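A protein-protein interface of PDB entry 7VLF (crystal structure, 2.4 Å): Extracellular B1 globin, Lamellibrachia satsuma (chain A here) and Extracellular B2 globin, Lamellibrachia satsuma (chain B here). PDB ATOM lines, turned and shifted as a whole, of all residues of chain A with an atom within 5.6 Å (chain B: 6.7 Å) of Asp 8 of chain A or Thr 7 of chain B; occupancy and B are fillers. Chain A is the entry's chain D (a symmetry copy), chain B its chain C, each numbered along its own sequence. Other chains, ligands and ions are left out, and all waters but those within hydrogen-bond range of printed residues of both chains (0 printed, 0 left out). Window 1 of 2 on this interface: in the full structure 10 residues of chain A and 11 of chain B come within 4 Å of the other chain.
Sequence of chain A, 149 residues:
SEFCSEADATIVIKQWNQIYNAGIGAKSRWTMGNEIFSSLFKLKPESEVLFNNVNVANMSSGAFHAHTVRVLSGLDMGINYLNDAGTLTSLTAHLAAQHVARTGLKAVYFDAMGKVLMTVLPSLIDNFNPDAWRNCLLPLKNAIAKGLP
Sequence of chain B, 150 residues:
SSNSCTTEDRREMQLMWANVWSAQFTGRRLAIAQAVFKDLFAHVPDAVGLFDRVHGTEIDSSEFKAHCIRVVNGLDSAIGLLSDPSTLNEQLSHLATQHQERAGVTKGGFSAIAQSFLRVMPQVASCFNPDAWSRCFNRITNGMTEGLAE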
ATOM      1  N   CYS A   4      13.431  19.553  -1.566  1.00  0.00           N
ATOM      2  CA  CYS A   4      12.331  18.620  -1.358  1.00  0.00           C
ATOM      3  C   CYS A   4      11.595  19.007  -0.084  1.00  0.00           C
ATOM      4  O   CYS A   4      12.128  19.723   0.769  1.00  0.00           O
ATOM      5  CB  CYS A   4      12.819  17.167  -1.290  1.00  0.00           C
ATOM      6  SG  CYS A   4      13.962  16.771   0.064  1.00  0.00           S
ATOM      7  N   SER A   5      10.359  18.526   0.026  1.00  0.00           N
ATOM      8  CA  SER A   5       9.510  18.875   1.155  1.00  0.00           C
ATOM      9  C   SER A   5      10.118  18.378   2.463  1.00  0.00           C
ATOM     10  O   SER A   5      10.935  17.455   2.491  1.00  0.00           O
ATOM     11  CB  SER A   5       8.113  18.281   0.978  1.00  0.00           C
ATOM     12  OG  SER A   5       8.142  16.872   1.128  1.00  0.00           O
ATOM     13  N   GLU A   6       9.705  19.018   3.561  1.00  0.00           N
ATOM     14  CA  GLU A   6      10.197  18.629   4.879  1.00  0.00           C
ATOM     15  C   GLU A   6       9.895  17.163   5.167  1.00  0.00           C
ATOM     16  O   GLU A   6      10.764  16.418   5.632  1.00  0.00           O
ATOM     17  CB  GLU A   6       9.581  19.521   5.957  1.00  0.00           C
ATOM     18  CG  GLU A   6       9.824  19.013   7.370  1.00  0.00           C
ATOM     19  CD  GLU A   6       8.896  19.640   8.390  1.00  0.00           C
ATOM     20  OE1 GLU A   6       8.738  20.878   8.371  1.00  0.00           O
ATOM     21  OE2 GLU A   6       8.320  18.892   9.209  1.00  0.00           O
ATOM     22  N   ALA A   7       8.659  16.735   4.893  1.00  0.00           N
ATOM     23  CA  ALA A   7       8.282  15.346   5.137  1.00  0.00           C
ATOM     24  C   ALA A   7       9.141  14.390   4.320  1.00  0.00           C
ATOM     25  O   ALA A   7       9.612  13.371   4.837  1.00  0.00           O
ATOM     26  CB  ALA A   7       6.800  15.144   4.822  1.00  0.00           C
ATOM     27  N   ASP A   8       9.360  14.702   3.039  1.00  0.00           N
ATOM     28  CA  ASP A   8      10.268  13.896   2.233  1.00  0.00           C
ATOM     29  C   ASP A   8      11.695  13.993   2.757  1.00  0.00           C
ATOM     30  O   ASP A   8      12.399  12.983   2.860  1.00  0.00           O
ATOM     31  CB  ASP A   8      10.204  14.331   0.767  1.00  0.00           C
ATOM     32  CG  ASP A   8       8.924  13.894   0.086  1.00  0.00           C
ATOM     33  OD1 ASP A   8       8.393  12.823   0.445  1.00  0.00           O
ATOM     34  OD2 ASP A   8       8.454  14.619  -0.815  1.00  0.00           O
ATOM     35  N   ALA A   9      12.138  15.207   3.094  1.00  0.00           N
ATOM     36  CA  ALA A   9      13.476  15.372   3.653  1.00  0.00           C
ATOM     37  C   ALA A   9      13.603  14.658   4.991  1.00  0.00           C
ATOM     38  O   ALA A   9      14.657  14.089   5.300  1.00  0.00           O
ATOM     39  CB  ALA A   9      13.809  16.855   3.802  1.00  0.00           C
ATOM     40  N   THR A  10      12.539  14.673   5.796  1.00  0.00           N
ATOM     41  CA  THR A  10      12.572  13.977   7.079  1.00  0.00           C
ATOM     42  C   THR A  10      12.745  12.476   6.884  1.00  0.00           C
ATOM     43  O   THR A  10      13.447  11.818   7.659  1.00  0.00           O
ATOM     44  CB  THR A  10      11.299  14.272   7.872  1.00  0.00           C
ATOM     45  OG1 THR A  10      11.126  15.691   7.988  1.00  0.00           O
ATOM     46  CG2 THR A  10      11.380  13.665   9.263  1.00  0.00           C
ATOM     47  N   ILE A  11      12.113  11.921   5.849  1.00  0.00           N
ATOM     48  CA  ILE A  11      12.241  10.493   5.579  1.00  0.00           C
ATOM     49  C   ILE A  11      13.667  10.151   5.167  1.00  0.00           C
ATOM     50  O   ILE A  11      14.212   9.115   5.566  1.00  0.00           O
ATOM     51  CB  ILE A  11      11.220  10.060   4.509  1.00  0.00           C
ATOM     52  CG1 ILE A  11       9.793  10.198   5.043  1.00  0.00           C
ATOM     53  CG2 ILE A  11      11.484   8.630   4.060  1.00  0.00           C
ATOM     54  CD1 ILE A  11       8.727   9.821   4.037  1.00  0.00           C
ATOM     55  N   VAL A  12      14.299  11.019   4.377  1.00  0.00           N
ATOM     56  CA  VAL A  12      15.640  10.731   3.877  1.00  0.00           C
ATOM     57  C   VAL A  12      16.659  10.790   5.010  1.00  0.00           C
ATOM     58  O   VAL A  12      17.505   9.900   5.149  1.00  0.00           O
ATOM     59  CB  VAL A  12      16.007  11.698   2.738  1.00  0.00           C
ATOM     60  CG1 VAL A  12      17.424  11.438   2.262  1.00  0.00           C
ATOM     61  CG2 VAL A  12      15.023  11.556   1.590  1.00  0.00           C
ATOM     62  N   ILE A  13      16.593  11.839   5.835  1.00  0.00           N
ATOM     63  CA  ILE A  13      17.593  12.025   6.884  1.00  0.00           C
ATOM     64  C   ILE A  13      17.534  10.887   7.892  1.00  0.00           C
ATOM     65  O   ILE A  13      18.571  10.377   8.335  1.00  0.00           O
ATOM     66  CB  ILE A  13      17.403  13.389   7.572  1.00  0.00           C
ATOM     67  CG1 ILE A  13      17.513  14.521   6.549  1.00  0.00           C
ATOM     68  CG2 ILE A  13      18.423  13.564   8.690  1.00  0.00           C
ATOM     69  CD1 ILE A  13      17.302  15.897   7.137  1.00  0.00           C
ATOM     70  N   ALA A 132      10.741   9.338  -1.988  1.00  0.00           N
ATOM     71  CA  ALA A 132      11.249  10.432  -1.166  1.00  0.00           C
ATOM     72  C   ALA A 132      12.736  10.658  -1.403  1.00  0.00           C
ATOM     73  O   ALA A 132      13.210  11.800  -1.384  1.00  0.00           O
ATOM     74  CB  ALA A 132      10.975  10.151   0.311  1.00  0.00           C
ATOM     75  N   ASN A 135      13.007  12.272  -4.713  1.00  0.00           N
ATOM     76  CA  ASN A 135      12.588  13.665  -4.605  1.00  0.00           C
ATOM     77  C   ASN A 135      13.666  14.531  -3.962  1.00  0.00           C
ATOM     78  O   ASN A 135      13.734  15.734  -4.239  1.00  0.00           O
ATOM     79  CB  ASN A 135      11.284  13.764  -3.813  1.00  0.00           C
ATOM     80  CG  ASN A 135      10.125  13.081  -4.512  1.00  0.00           C
ATOM     81  OD1 ASN A 135      10.063  13.041  -5.742  1.00  0.00           O
ATOM     82  ND2 ASN A 135       9.202  12.534  -3.730  1.00  0.00           N
ATOM     83  N   CYS A 136      14.513  13.949  -3.109  1.00  0.00           N
ATOM     84  CA  CYS A 136      15.517  14.723  -2.390  1.00  0.00           C
ATOM     85  C   CYS A 136      16.921  14.567  -2.956  1.00  0.00           C
ATOM     86  O   CYS A 136      17.749  15.464  -2.763  1.00  0.00           O
ATOM     87  CB  CYS A 136      15.544  14.333  -0.905  1.00  0.00           C
ATOM     88  SG  CYS A 136      14.058  14.739   0.047  1.00  0.00           S
ATOM     89  N   SER B   4       7.073  17.327  -7.990  1.00  0.00           N
ATOM     90  CA  SER B   4       7.184  15.965  -7.490  1.00  0.00           C
ATOM     91  C   SER B   4       6.053  15.655  -6.520  1.00  0.00           C
ATOM     92  O   SER B   4       5.549  16.532  -5.814  1.00  0.00           O
ATOM     93  CB  SER B   4       8.528  15.751  -6.792  1.00  0.00           C
ATOM     94  OG  SER B   4       9.606  16.026  -7.667  1.00  0.00           O
ATOM     95  N   CYS B   5       5.652  14.388  -6.495  1.00  0.00           N
ATOM     96  CA  CYS B   5       4.607  13.919  -5.588  1.00  0.00           C
ATOM     97  C   CYS B   5       5.180  13.842  -4.179  1.00  0.00           C
ATOM     98  O   CYS B   5       5.867  12.881  -3.823  1.00  0.00           O
ATOM     99  CB  CYS B   5       4.075  12.567  -6.050  1.00  0.00           C
ATOM    100  SG  CYS B   5       2.992  11.731  -4.868  1.00  0.00           S
ATOM    101  N   THR B   6       4.908  14.866  -3.373  1.00  0.00           N
ATOM    102  CA  THR B   6       5.443  14.941  -2.026  1.00  0.00           C
ATOM    103  C   THR B   6       4.726  13.948  -1.107  1.00  0.00           C
ATOM    104  O   THR B   6       3.669  13.393  -1.430  1.00  0.00           O
ATOM    105  CB  THR B   6       5.315  16.362  -1.474  1.00  0.00           C
ATOM    106  OG1 THR B   6       3.950  16.788  -1.535  1.00  0.00           O
ATOM    107  CG2 THR B   6       6.175  17.328  -2.277  1.00  0.00           C
ATOM    108  N   THR B   7       5.339  13.711   0.056  1.00  0.00           N
ATOM    109  CA  THR B   7       4.665  12.965   1.113  1.00  0.00           C
ATOM    110  C   THR B   7       3.420  13.699   1.589  1.00  0.00           C
ATOM    111  O   THR B   7       2.430  13.065   1.969  1.00  0.00           O
ATOM    112  CB  THR B   7       5.627  12.726   2.281  1.00  0.00           C
ATOM    113  OG1 THR B   7       6.804  12.068   1.798  1.00  0.00           O
ATOM    114  CG2 THR B   7       4.975  11.858   3.356  1.00  0.00           C
ATOM    115  N   GLU B   8       3.441  15.033   1.548  1.00  0.00           N
ATOM    116  CA  GLU B   8       2.271  15.806   1.947  1.00  0.00           C
ATOM    117  C   GLU B   8       1.074  15.482   1.062  1.00  0.00           C
ATOM    118  O   GLU B   8      -0.031  15.230   1.556  1.00  0.00           O
ATOM    119  CB  GLU B   8       2.591  17.298   1.894  1.00  0.00           C
ATOM    120  CG  GLU B   8       3.538  17.769   2.981  1.00  0.00           C
ATOM    121  CD  GLU B   8       4.994  17.460   2.686  1.00  0.00           C
ATOM    122  OE1 GLU B   8       5.271  16.670   1.757  1.00  0.00           O
ATOM    123  OE2 GLU B   8       5.865  18.017   3.384  1.00  0.00           O
ATOM    124  N   ASP B   9       1.279  15.482  -0.257  1.00  0.00           N
ATOM    125  CA  ASP B   9       0.194  15.161  -1.177  1.00  0.00           C
ATOM    126  C   ASP B   9      -0.257  13.719  -1.007  1.00  0.00           C
ATOM    127  O   ASP B   9      -1.456  13.424  -1.074  1.00  0.00           O
ATOM    128  CB  ASP B   9       0.640  15.402  -2.615  1.00  0.00           C
ATOM    129  CG  ASP B   9       1.222  16.776  -2.818  1.00  0.00           C
ATOM    130  OD1 ASP B   9       0.886  17.683  -2.030  1.00  0.00           O
ATOM    131  OD2 ASP B   9       2.023  16.945  -3.763  1.00  0.00           O
ATOM    132  N   ARG B  10       0.695  12.805  -0.807  1.00  0.00           N
ATOM    133  CA  ARG B  10       0.372  11.402  -0.564  1.00  0.00           C
ATOM    134  C   ARG B  10      -0.622  11.256   0.579  1.00  0.00           C
ATOM    135  O   ARG B  10      -1.658  10.595   0.439  1.00  0.00           O
ATOM    136  CB  ARG B  10       1.655  10.629  -0.273  1.00  0.00           C
ATOM    137  CG  ARG B  10       2.511  10.425  -1.501  1.00  0.00           C
ATOM    138  CD  ARG B  10       3.960  10.182  -1.142  1.00  0.00           C
ATOM    139  NE  ARG B  10       4.845  10.509  -2.255  1.00  0.00           N
ATOM    140  CZ  ARG B  10       5.300   9.623  -3.133  1.00  0.00           C
ATOM    141  NH1 ARG B  10       4.959   8.345  -3.025  1.00  0.00           N
ATOM    142  NH2 ARG B  10       6.096  10.015  -4.115  1.00  0.00           N
ATOM    143  N   ARG B  11      -0.319  11.879   1.720  1.00  0.00           N
ATOM    144  CA  ARG B  11      -1.270  11.932   2.826  1.00  0.00           C
ATOM    145  C   ARG B  11      -2.559  12.615   2.394  1.00  0.00           C
ATOM    146  O   ARG B  11      -3.658  12.104   2.638  1.00  0.00           O
ATOM    147  CB  ARG B  11      -0.665  12.676   4.018  1.00  0.00           C
ATOM    148  CG  ARG B  11       0.567  12.027   4.618  1.00  0.00           C
ATOM    149  CD  ARG B  11       0.825  12.528   6.026  1.00  0.00           C
ATOM    150  NE  ARG B  11       2.056  11.988   6.595  1.00  0.00           N
ATOM    151  CZ  ARG B  11       2.170  10.771   7.118  1.00  0.00           C
ATOM    152  NH1 ARG B  11       3.330  10.374   7.619  1.00  0.00           N
ATOM    153  NH2 ARG B  11       1.128   9.952   7.134  1.00  0.00           N
ATOM    154  N   GLU B  12      -2.439  13.779   1.747  1.00  0.00           N
ATOM    155  CA  GLU B  12      -3.615  14.531   1.324  1.00  0.00           C
ATOM    156  C   GLU B  12      -4.425  13.761   0.289  1.00  0.00           C
ATOM    157  O   GLU B  12      -5.659  13.721   0.360  1.00  0.00           O
ATOM    158  CB  GLU B  12      -3.186  15.893   0.774  1.00  0.00           C
ATOM    159  CG  GLU B  12      -4.313  16.690   0.152  1.00  0.00           C
ATOM    160  CD  GLU B  12      -3.956  18.147  -0.056  1.00  0.00           C
ATOM    161  OE1 GLU B  12      -4.864  18.997   0.050  1.00  0.00           O
ATOM    162  OE2 GLU B  12      -2.772  18.446  -0.323  1.00  0.00           O
ATOM    163  N   GLN B  14      -4.337  10.376  -0.345  1.00  0.00           N
ATOM    164  CA  GLN B  14      -4.876   9.144   0.222  1.00  0.00           C
ATOM    165  C   GLN B  14      -6.074   9.425   1.116  1.00  0.00           C
ATOM    166  O   GLN B  14      -7.067   8.689   1.086  1.00  0.00           O
ATOM    167  CB  GLN B  14      -3.796   8.409   1.016  1.00  0.00           C
ATOM    168  CG  GLN B  14      -2.736   7.733   0.173  1.00  0.00           C
ATOM    169  CD  GLN B  14      -1.594   7.194   1.009  1.00  0.00           C
ATOM    170  OE1 GLN B  14      -0.836   6.329   0.567  1.00  0.00           O
ATOM    171  NE2 GLN B  14      -1.463   7.705   2.227  1.00  0.00           N
ATOM    172  N   CYS B 136       0.768  13.799  -7.920  1.00  0.00           N
ATOM    173  CA  CYS B 136       0.885  12.373  -7.652  1.00  0.00           C
ATOM    174  C   CYS B 136       0.197  11.526  -8.711  1.00  0.00           C
ATOM    175  O   CYS B 136       0.650  10.410  -8.987  1.00  0.00           O
ATOM    176  CB  CYS B 136       0.321  12.042  -6.269  1.00  0.00           C
ATOM    177  SG  CYS B 136       1.257  12.788  -4.922  1.00  0.00           S
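Asp 8 of chain A touches two residues of chain B. Of chain A, only Ala 7 (3.7 Å), Asp 8 (2.2 Å) and Ile 11 (3.7 Å) come within 4 Å of Thr 7 of chain B. Printed residues of chain B within 4 Å of Glu 6 of chain A: Glu 8 (3.97 Å). Printed residues of chain B within 4 Å of Asn 135 of chain A: Ser 4 (3.3 Å) and Cys 5 (3.4 Å). Cys 4 of chain A touches none of the printed residues of chain B. Val 12 of chain A touches none of the printed residues of chain B. The nearest residue of chain A that does not touch Thr 7 of chain B is Ser 5 of chain A (4.4 Å).
The backbone carbonyl oxygen (O) of Cys 5 of chain B sits at hydrogen-bond distance from the guanidinium group (NH2) of Arg 10 of chain B. The side-chain sulfur (SG) of Cys 5 of chain B forms a disulfide with the side-chain sulfur (SG) of Cys 136 of chain B. The side-chain hydroxyl (OG1) of Thr 6 of chain B is in hydrogen-bond range of the side-chain carboxylate (OD2) of Asp 9 of chain B. O of Thr 6 of chain B lies close to NE of Arg 10 of chain B. The side-chain carboxylate (OD2) of Asp 8 of chain A is in hydrogen-bond range of the side-chain hydroxyl (OG) of Ser 5 of chain A (3.0 Å). SG of Cys 136 of chain A forms a disulfide with SG of Cys 4 of chain A, at 2.0 Å.
Printed residues of chain A that touch a printed residue of chain B: Ser 5, Glu 6, Ala 7, Asp 8, Ile 11 and Asn 135. Among the printed residues, 10 pairs touch across the chains.
ND2 of Asn 135 of chain A lies within hydrogen-bond range of O of Cys 5 of chain B, 3.4 Å away. The side-chain carboxylate of Asp 8 of chain A lies within hydrogen-bond range of the backbone NH of Thr 7 of chain B (3.2 Å). The side-chain carboxylate (OE1) of Glu 8 of chain B lies within hydrogen-bond range of the side-chain hydroxyl (OG) of Ser 5 of chain A, 2.9 Å away. The side-chain carboxylate (OE2) of Glu 8 of chain B sits close to the backbone NH (N) of Ala 7 of chain A.
Among the printed residues, pairs that only touch across the chains: Asp 8 of chain A with Thr 6 of chain B (3.3 Å), Asn 135 of chain A with Ser 4 of chain B (3.3 Å), Ala 7 of chain A with Thr 7 of chain B (3.7 Å), Ile 11 of chain A with Thr 7 of chain B (3.7 Å), Ser 5 of chain A with Thr 6 of chain B (3.9 Å) and Glu 6 of chain A with Glu 8 of chain B (3.97 Å).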
